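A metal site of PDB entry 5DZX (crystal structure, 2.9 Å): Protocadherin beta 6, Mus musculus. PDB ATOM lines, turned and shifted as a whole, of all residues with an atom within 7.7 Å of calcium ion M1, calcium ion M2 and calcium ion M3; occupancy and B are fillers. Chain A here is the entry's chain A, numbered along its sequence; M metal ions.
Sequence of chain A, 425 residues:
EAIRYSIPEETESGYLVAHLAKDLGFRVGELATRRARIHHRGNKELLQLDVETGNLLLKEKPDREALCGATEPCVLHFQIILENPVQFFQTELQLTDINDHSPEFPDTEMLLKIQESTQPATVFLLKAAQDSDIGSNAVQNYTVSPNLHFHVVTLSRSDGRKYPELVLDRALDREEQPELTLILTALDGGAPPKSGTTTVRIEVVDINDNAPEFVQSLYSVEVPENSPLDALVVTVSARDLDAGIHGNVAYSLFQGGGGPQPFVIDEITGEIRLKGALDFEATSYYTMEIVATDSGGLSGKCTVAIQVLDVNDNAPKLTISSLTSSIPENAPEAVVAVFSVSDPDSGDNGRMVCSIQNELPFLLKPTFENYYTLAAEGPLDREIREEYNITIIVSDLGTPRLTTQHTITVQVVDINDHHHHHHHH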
ATOM      1  N   GLU A   9     -29.493   5.818  24.205  1.00  0.00           N
ATOM      2  CA  GLU A   9     -29.284   4.945  25.349  1.00  0.00           C
ATOM      3  C   GLU A   9     -30.440   5.061  26.333  1.00  0.00           C
ATOM      4  O   GLU A   9     -31.104   6.099  26.408  1.00  0.00           O
ATOM      5  CB  GLU A   9     -27.957   5.287  26.027  1.00  0.00           C
ATOM      6  CG  GLU A   9     -27.622   4.449  27.242  1.00  0.00           C
ATOM      7  CD  GLU A   9     -26.740   5.185  28.219  1.00  0.00           C
ATOM      8  OE1 GLU A   9     -26.087   6.169  27.802  1.00  0.00           O
ATOM      9  OE2 GLU A   9     -26.695   4.791  29.401  1.00  0.00           O
ATOM     10  N   GLU A  10     -30.707   3.978  27.070  1.00  0.00           N
ATOM     11  CA  GLU A  10     -31.693   3.958  28.145  1.00  0.00           C
ATOM     12  C   GLU A  10     -33.112   4.264  27.656  1.00  0.00           C
ATOM     13  O   GLU A  10     -33.932   4.791  28.397  1.00  0.00           O
ATOM     14  CB  GLU A  10     -31.320   4.937  29.259  1.00  0.00           C
ATOM     15  CG  GLU A  10     -29.956   4.697  29.901  1.00  0.00           C
ATOM     16  CD  GLU A  10     -29.954   3.529  30.876  1.00  0.00           C
ATOM     17  OE1 GLU A  10     -30.983   2.835  31.003  1.00  0.00           O
ATOM     18  OE2 GLU A  10     -28.907   3.313  31.523  1.00  0.00           O
ATOM     19  N   PRO A  62     -31.519  -0.473  27.018  1.00  0.00           N
ATOM     20  CA  PRO A  62     -30.093  -0.544  26.669  1.00  0.00           C
ATOM     21  C   PRO A  62     -29.240   0.456  27.444  1.00  0.00           C
ATOM     22  O   PRO A  62     -29.493   1.649  27.426  1.00  0.00           O
ATOM     23  CB  PRO A  62     -30.101  -0.198  25.177  1.00  0.00           C
ATOM     24  CG  PRO A  62     -31.268   0.715  25.018  1.00  0.00           C
ATOM     25  CD  PRO A  62     -32.302   0.279  26.027  1.00  0.00           C
ATOM     26  N   ASP A  63     -28.218  -0.062  28.124  1.00  0.00           N
ATOM     27  CA  ASP A  63     -27.276   0.783  28.845  1.00  0.00           C
ATOM     28  C   ASP A  63     -25.934   0.803  28.130  1.00  0.00           C
ATOM     29  O   ASP A  63     -25.243  -0.208  28.054  1.00  0.00           O
ATOM     30  CB  ASP A  63     -27.111   0.302  30.285  1.00  0.00           C
ATOM     31  CG  ASP A  63     -26.263   1.234  31.119  1.00  0.00           C
ATOM     32  OD1 ASP A  63     -26.253   2.446  30.824  1.00  0.00           O
ATOM     33  OD2 ASP A  63     -25.586   0.751  32.060  1.00  0.00           O
ATOM     34  N   ARG A  64     -25.574   1.974  27.596  1.00  0.00           N
ATOM     35  CA  ARG A  64     -24.351   2.134  26.826  1.00  0.00           C
ATOM     36  C   ARG A  64     -23.118   1.779  27.656  1.00  0.00           C
ATOM     37  O   ARG A  64     -22.271   0.988  27.221  1.00  0.00           O
ATOM     38  CB  ARG A  64     -24.243   3.576  26.302  1.00  0.00           C
ATOM     39  CG  ARG A  64     -23.521   3.729  24.965  1.00  0.00           C
ATOM     40  CD  ARG A  64     -22.016   3.484  25.071  1.00  0.00           C
ATOM     41  NE  ARG A  64     -21.439   4.124  26.255  1.00  0.00           N
ATOM     42  CZ  ARG A  64     -21.089   5.400  26.305  1.00  0.00           C
ATOM     43  NH1 ARG A  64     -20.560   5.909  27.414  1.00  0.00           N
ATOM     44  NH2 ARG A  64     -21.257   6.185  25.250  1.00  0.00           N
ATOM     45  N   GLU A  65     -23.030   2.346  28.848  1.00  0.00           N
ATOM     46  CA  GLU A  65     -21.854   2.199  29.700  1.00  0.00           C
ATOM     47  C   GLU A  65     -21.644   0.769  30.195  1.00  0.00           C
ATOM     48  O   GLU A  65     -20.585   0.434  30.718  1.00  0.00           O
ATOM     49  CB  GLU A  65     -21.947   3.145  30.897  1.00  0.00           C
ATOM     50  CG  GLU A  65     -21.898   4.633  30.550  1.00  0.00           C
ATOM     51  CD  GLU A  65     -23.226   5.172  30.058  1.00  0.00           C
ATOM     52  OE1 GLU A  65     -24.271   4.602  30.430  1.00  0.00           O
ATOM     53  OE2 GLU A  65     -23.219   6.160  29.300  1.00  0.00           O
ATOM     54  N   ALA A  66     -22.663  -0.076  30.026  1.00  0.00           N
ATOM     55  CA  ALA A  66     -22.595  -1.453  30.509  1.00  0.00           C
ATOM     56  C   ALA A  66     -22.501  -2.454  29.369  1.00  0.00           C
ATOM     57  O   ALA A  66     -22.207  -3.631  29.589  1.00  0.00           O
ATOM     58  CB  ALA A  66     -23.808  -1.763  31.377  1.00  0.00           C
ATOM     59  N   THR A  96     -26.942   5.612  20.772  1.00  0.00           N
ATOM     60  CA  THR A  96     -26.499   6.984  20.979  1.00  0.00           C
ATOM     61  C   THR A  96     -26.358   7.272  22.469  1.00  0.00           C
ATOM     62  O   THR A  96     -27.255   6.959  23.258  1.00  0.00           O
ATOM     63  CB  THR A  96     -27.456   8.002  20.346  1.00  0.00           C
ATOM     64  OG1 THR A  96     -27.591   7.739  18.944  1.00  0.00           O
ATOM     65  CG2 THR A  96     -26.926   9.421  20.526  1.00  0.00           C
ATOM     66  N   ASP A  97     -25.242   7.884  22.848  1.00  0.00           N
ATOM     67  CA  ASP A  97     -24.974   8.199  24.246  1.00  0.00           C
ATOM     68  C   ASP A  97     -25.808   9.380  24.720  1.00  0.00           C
ATOM     69  O   ASP A  97     -25.834  10.433  24.077  1.00  0.00           O
ATOM     70  CB  ASP A  97     -23.495   8.493  24.457  1.00  0.00           C
ATOM     71  CG  ASP A  97     -23.171   8.795  25.903  1.00  0.00           C
ATOM     72  OD1 ASP A  97     -23.792   8.166  26.792  1.00  0.00           O
ATOM     73  OD2 ASP A  97     -22.327   9.677  26.159  1.00  0.00           O
ATOM     74  N   ILE A  98     -26.463   9.211  25.857  1.00  0.00           N
ATOM     75  CA  ILE A  98     -27.226  10.288  26.463  1.00  0.00           C
ATOM     76  C   ILE A  98     -26.621  10.653  27.827  1.00  0.00           C
ATOM     77  O   ILE A  98     -26.216   9.769  28.580  1.00  0.00           O
ATOM     78  CB  ILE A  98     -28.704   9.904  26.620  1.00  0.00           C
ATOM     79  CG1 ILE A  98     -28.842   8.516  27.251  1.00  0.00           C
ATOM     80  CG2 ILE A  98     -29.396   9.918  25.261  1.00  0.00           C
ATOM     81  CD1 ILE A  98     -29.239   8.536  28.709  1.00  0.00           C
ATOM     82  N   ASN A  99     -26.551  11.951  28.108  1.00  0.00           N
ATOM     83  CA  ASN A  99     -25.905  12.440  29.320  1.00  0.00           C
ATOM     84  C   ASN A  99     -26.698  12.095  30.580  1.00  0.00           C
ATOM     85  O   ASN A  99     -27.503  12.901  31.046  1.00  0.00           O
ATOM     86  CB  ASN A  99     -25.710  13.955  29.223  1.00  0.00           C
ATOM     87  CG  ASN A  99     -24.802  14.495  30.314  1.00  0.00           C
ATOM     88  OD1 ASN A  99     -23.974  13.775  30.853  1.00  0.00           O
ATOM     89  ND2 ASN A  99     -24.965  15.773  30.641  1.00  0.00           N
ATOM     90  N   ASP A 100     -26.444  10.924  31.140  1.00  0.00           N
ATOM     91  CA  ASP A 100     -27.157  10.471  32.321  1.00  0.00           C
ATOM     92  C   ASP A 100     -26.215  10.224  33.492  1.00  0.00           C
ATOM     93  O   ASP A 100     -26.547   9.506  34.433  1.00  0.00           O
ATOM     94  CB  ASP A 100     -27.964   9.195  32.002  1.00  0.00           C
ATOM     95  CG  ASP A 100     -27.095   8.068  31.473  1.00  0.00           C
ATOM     96  OD1 ASP A 100     -25.964   8.334  31.001  1.00  0.00           O
ATOM     97  OD2 ASP A 100     -27.547   6.903  31.502  1.00  0.00           O
ATOM     98  N   HIS A 101     -25.040  10.839  33.435  1.00  0.00           N
ATOM     99  CA  HIS A 101     -24.067  10.747  34.517  1.00  0.00           C
ATOM    100  C   HIS A 101     -23.470  12.101  34.860  1.00  0.00           C
ATOM    101  O   HIS A 101     -23.037  12.840  33.975  1.00  0.00           O
ATOM    102  CB  HIS A 101     -22.950   9.758  34.148  1.00  0.00           C
ATOM    103  CG  HIS A 101     -23.376   8.328  34.194  1.00  0.00           C
ATOM    104  ND1 HIS A 101     -24.295   7.792  33.315  1.00  0.00           N
ATOM    105  CD2 HIS A 101     -23.011   7.324  35.026  1.00  0.00           C
ATOM    106  CE1 HIS A 101     -24.472   6.518  33.603  1.00  0.00           C
ATOM    107  NE2 HIS A 101     -23.710   6.205  34.630  1.00  0.00           N
ATOM    108  N   SER A 102     -23.434  12.428  36.147  1.00  0.00           N
ATOM    109  CA  SER A 102     -22.879  13.690  36.591  1.00  0.00           C
ATOM    110  C   SER A 102     -21.388  13.554  36.904  1.00  0.00           C
ATOM    111  O   SER A 102     -20.969  12.559  37.487  1.00  0.00           O
ATOM    112  CB  SER A 102     -23.623  14.209  37.821  1.00  0.00           C
ATOM    113  OG  SER A 102     -25.011  14.339  37.542  1.00  0.00           O
ATOM    114  N   PRO A 103     -20.592  14.566  36.515  1.00  0.00           N
ATOM    115  CA  PRO A 103     -19.166  14.584  36.844  1.00  0.00           C
ATOM    116  C   PRO A 103     -18.964  14.437  38.344  1.00  0.00           C
ATOM    117  O   PRO A 103     -19.614  15.116  39.129  1.00  0.00           O
ATOM    118  CB  PRO A 103     -18.711  15.961  36.364  1.00  0.00           C
ATOM    119  CG  PRO A 103     -19.658  16.302  35.270  1.00  0.00           C
ATOM    120  CD  PRO A 103     -20.984  15.740  35.718  1.00  0.00           C
ATOM    121  N   GLN A 130     -14.254  11.836  37.362  1.00  0.00           N
ATOM    122  CA  GLN A 130     -14.631  10.668  36.587  1.00  0.00           C
ATOM    123  C   GLN A 130     -16.052  10.791  36.037  1.00  0.00           C
ATOM    124  O   GLN A 130     -16.980  11.160  36.750  1.00  0.00           O
ATOM    125  CB  GLN A 130     -14.479   9.398  37.431  1.00  0.00           C
ATOM    126  CG  GLN A 130     -15.029   9.512  38.843  1.00  0.00           C
ATOM    127  CD  GLN A 130     -14.454   8.464  39.770  1.00  0.00           C
ATOM    128  OE1 GLN A 130     -13.541   7.730  39.404  1.00  0.00           O
ATOM    129  NE2 GLN A 130     -14.979   8.394  40.993  1.00  0.00           N
ATOM    130  N   ASP A 131     -16.201  10.466  34.764  1.00  0.00           N
ATOM    131  CA  ASP A 131     -17.500  10.495  34.098  1.00  0.00           C
ATOM    132  C   ASP A 131     -17.663   9.260  33.216  1.00  0.00           C
ATOM    133  O   ASP A 131     -16.770   8.931  32.440  1.00  0.00           O
ATOM    134  CB  ASP A 131     -17.655  11.776  33.263  1.00  0.00           C
ATOM    135  CG  ASP A 131     -19.097  12.093  32.938  1.00  0.00           C
ATOM    136  OD1 ASP A 131     -19.892  11.142  32.762  1.00  0.00           O
ATOM    137  OD2 ASP A 131     -19.444  13.285  32.855  1.00  0.00           O
ATOM    138  N   SER A 132     -18.797   8.588  33.347  1.00  0.00           N
ATOM    139  CA  SER A 132     -19.065   7.381  32.566  1.00  0.00           C
ATOM    140  C   SER A 132     -19.387   7.715  31.115  1.00  0.00           C
ATOM    141  O   SER A 132     -19.059   6.950  30.217  1.00  0.00           O
ATOM    142  CB  SER A 132     -20.221   6.591  33.186  1.00  0.00           C
ATOM    143  OG  SER A 132     -19.886   6.116  34.481  1.00  0.00           O
ATOM    144  N   ASP A 133     -20.013   8.868  30.898  1.00  0.00           N
ATOM    145  CA  ASP A 133     -20.376   9.301  29.551  1.00  0.00           C
ATOM    146  C   ASP A 133     -19.145   9.641  28.722  1.00  0.00           C
ATOM    147  O   ASP A 133     -18.033   9.725  29.249  1.00  0.00           O
ATOM    148  CB  ASP A 133     -21.313  10.515  29.621  1.00  0.00           C
ATOM    149  CG  ASP A 133     -22.601  10.215  30.358  1.00  0.00           C
ATOM    150  OD1 ASP A 133     -23.094   9.069  30.267  1.00  0.00           O
ATOM    151  OD2 ASP A 133     -23.121  11.132  31.031  1.00  0.00           O
ATOM    152  N   ILE A 134     -19.345   9.824  27.422  1.00  0.00           N
ATOM    153  CA  ILE A 134     -18.242  10.145  26.523  1.00  0.00           C
ATOM    154  C   ILE A 134     -18.611  11.316  25.621  1.00  0.00           C
ATOM    155  O   ILE A 134     -19.747  11.782  25.616  1.00  0.00           O
ATOM    156  CB  ILE A 134     -17.829   8.928  25.663  1.00  0.00           C
ATOM    157  CG1 ILE A 134     -19.017   8.415  24.833  1.00  0.00           C
ATOM    158  CG2 ILE A 134     -17.277   7.811  26.529  1.00  0.00           C
ATOM    159  CD1 ILE A 134     -19.024   8.863  23.387  1.00  0.00           C
ATOM    160  N   SER A 136     -19.362  14.730  24.003  1.00  0.00           N
ATOM    161  CA  SER A 136     -19.905  15.992  24.504  1.00  0.00           C
ATOM    162  C   SER A 136     -20.572  15.814  25.868  1.00  0.00           C
ATOM    163  O   SER A 136     -20.756  16.787  26.605  1.00  0.00           O
ATOM    164  CB  SER A 136     -20.905  16.571  23.499  1.00  0.00           C
ATOM    165  OG  SER A 136     -21.479  17.773  23.971  1.00  0.00           O
ATOM    166  N   ASN A 137     -20.946  14.589  26.198  1.00  0.00           N
ATOM    167  CA  ASN A 137     -21.615  14.295  27.464  1.00  0.00           C
ATOM    168  C   ASN A 137     -20.638  14.042  28.608  1.00  0.00           C
ATOM    169  O   ASN A 137     -21.057  13.844  29.751  1.00  0.00           O
ATOM    170  CB  ASN A 137     -22.547  13.104  27.306  1.00  0.00           C
ATOM    171  CG  ASN A 137     -23.754  13.417  26.444  1.00  0.00           C
ATOM    172  OD1 ASN A 137     -24.197  14.572  26.383  1.00  0.00           O
ATOM    173  ND2 ASN A 137     -24.294  12.410  25.769  1.00  0.00           N
ATOM    174  N   ALA A 138     -19.352  14.038  28.298  1.00  0.00           N
ATOM    175  CA  ALA A 138     -18.329  13.880  29.318  1.00  0.00           C
ATOM    176  C   ALA A 138     -17.918  15.246  29.870  1.00  0.00           C
ATOM    177  O   ALA A 138     -18.443  16.270  29.454  1.00  0.00           O
ATOM    178  CB  ALA A 138     -17.120  13.146  28.767  1.00  0.00           C
ATOM    179  N   VAL A 139     -16.972  15.240  30.798  1.00  0.00           N
ATOM    180  CA  VAL A 139     -16.431  16.470  31.358  1.00  0.00           C
ATOM    181  C   VAL A 139     -15.818  17.309  30.238  1.00  0.00           C
ATOM    182  O   VAL A 139     -15.074  16.784  29.410  1.00  0.00           O
ATOM    183  CB  VAL A 139     -15.386  16.182  32.443  1.00  0.00           C
ATOM    184  CG1 VAL A 139     -14.791  17.474  32.956  1.00  0.00           C
ATOM    185  CG2 VAL A 139     -16.014  15.393  33.576  1.00  0.00           C
ATOM    186  N   ASP A 188     -19.817  19.726  32.808  1.00  0.00           N
ATOM    187  CA  ASP A 188     -20.156  18.831  31.729  1.00  0.00           C
ATOM    188  C   ASP A 188     -20.446  19.630  30.461  1.00  0.00           C
ATOM    189  O   ASP A 188     -20.801  20.806  30.521  1.00  0.00           O
ATOM    190  CB  ASP A 188     -21.363  17.977  32.118  1.00  0.00           C
ATOM    191  CG  ASP A 188     -21.493  16.726  31.292  1.00  0.00           C
ATOM    192  OD1 ASP A 188     -22.056  16.807  30.174  1.00  0.00           O
ATOM    193  OD2 ASP A 188     -21.046  15.660  31.754  1.00  0.00           O
ATOM    194  N   GLY A 189     -20.292  18.987  29.301  1.00  0.00           N
ATOM    195  CA  GLY A 189     -20.524  19.653  28.035  1.00  0.00           C
ATOM    196  C   GLY A 189     -21.966  19.606  27.562  1.00  0.00           C
ATOM    197  O   GLY A 189     -22.365  20.365  26.678  1.00  0.00           O
ATOM    198  N   GLY A 190     -22.748  18.712  28.156  1.00  0.00           N
ATOM    199  CA  GLY A 190     -24.137  18.533  27.776  1.00  0.00           C
ATOM    200  C   GLY A 190     -25.016  19.729  28.087  1.00  0.00           C
ATOM    201  O   GLY A 190     -24.605  20.661  28.787  1.00  0.00           O
ATOM    202  N   LYS A 194     -23.861  19.400  33.839  1.00  0.00           N
ATOM    203  CA  LYS A 194     -23.953  18.845  35.196  1.00  0.00           C
ATOM    204  C   LYS A 194     -22.694  19.159  36.000  1.00  0.00           C
ATOM    205  O   LYS A 194     -21.575  19.112  35.475  1.00  0.00           O
ATOM    206  CB  LYS A 194     -24.196  17.332  35.145  1.00  0.00           C
ATOM    207  CG  LYS A 194     -25.537  16.961  34.546  1.00  0.00           C
ATOM    208  CD  LYS A 194     -25.784  15.461  34.570  1.00  0.00           C
ATOM    209  CE  LYS A 194     -27.179  15.130  34.063  1.00  0.00           C
ATOM    210  NZ  LYS A 194     -27.486  13.683  34.138  1.00  0.00           N
HETATM  211 CA    CA M   1     -21.959  13.219  32.007  1.00  0.00          CA
HETATM  212 CA    CA M   2     -24.727   7.757  28.988  1.00  0.00          CA
HETATM  213 CA    CA M   3     -26.693   4.751  31.555  1.00  0.00          CA
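Of the 28 residues printed, 6 come within 4 Å of calcium ion M1.
O of Thr 96 is in hydrogen-bond range of N of Glu 9 (2.7 Å). The guanidinium group (NH1) of Arg 64 lies close to the side-chain carboxylate (OE2) of Glu 65 (3.3 Å). OD1 of Asp 100 lies close to ND1 of His 101 (2.9 Å). O of Asn 99 lies within hydrogen-bond range of NZ of Lys 194 (3.2 Å). The side-chain carboxylate (OD2) of Asp 97 is in hydrogen-bond range of the backbone NH (N) of Ile 134, at 3.2 Å. The backbone NH (N) of Asp 188 sits at hydrogen-bond distance from the backbone carbonyl oxygen (O) of Lys 194, at 3.3 Å. N of Gly 190 is in hydrogen-bond range of OD1 of Asp 188 (2.9 Å). The backbone carbonyl oxygen (O) of Pro 62 sits at hydrogen-bond distance from the backbone NH (N) of Glu 10, at 2.7 Å.
O of His 101 is bound to calcium ion M1, 2.3 Å away. Calcium ion M1 is bound by the side-chain amide oxygen (OD1) of Asn 99 (2.4 Å). Calcium ion M1 is bound by the backbone carbonyl oxygen (O) of Asn 137, at 2.5 Å. OD2 of Asp 133 is bound to calcium ion M1. Calcium ion M1 is bound by OD2 of Asp 188 (2.6 Å). Calcium ion M1 is bound by OD2 of Asp 131 (2.7 Å). Slightly farther from calcium ion M1 lies OD1 of Asp 131 (3.0 Å).
Calcium ion M3 is bound by OE2 of Glu 9, 2.2 Å away. OD2 of Asp 100 binds calcium ion M3 (2.3 Å). OD1 of Asp 63 binds calcium ion M3. OE2 of Glu 10 is bound to calcium ion M3. Calcium ion M3 is bound by OE1 of Glu 65. Calcium ion M3 has five donor atoms within binding distance.
OE2 of Glu 65 is bound to calcium ion M2, 2.2 Å away. Calcium ion M2 is bound by OE1 of Glu 9, 2.4 Å away. Calcium ion M2 is bound by OD1 of Asp 97, 2.4 Å away. The side-chain carboxylate (OD1) of Asp 100 is bound to calcium ion M2. OD1 of Asp 133 binds calcium ion M2 (2.5 Å). O of Ile 98 binds calcium ion M2, 2.5 Å away.
The nearest printed residue that does not touch calcium ion M3 is Arg 64 (5.0 Å).
Of the 28 residues printed, 6 come within 4 Å of calcium ion M2. Along chain A the residues within 4 Å of calcium ion M2 span positions 9 to 133. The nearest printed residue that does not touch calcium ion M2 is His 101 (4.3 Å).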
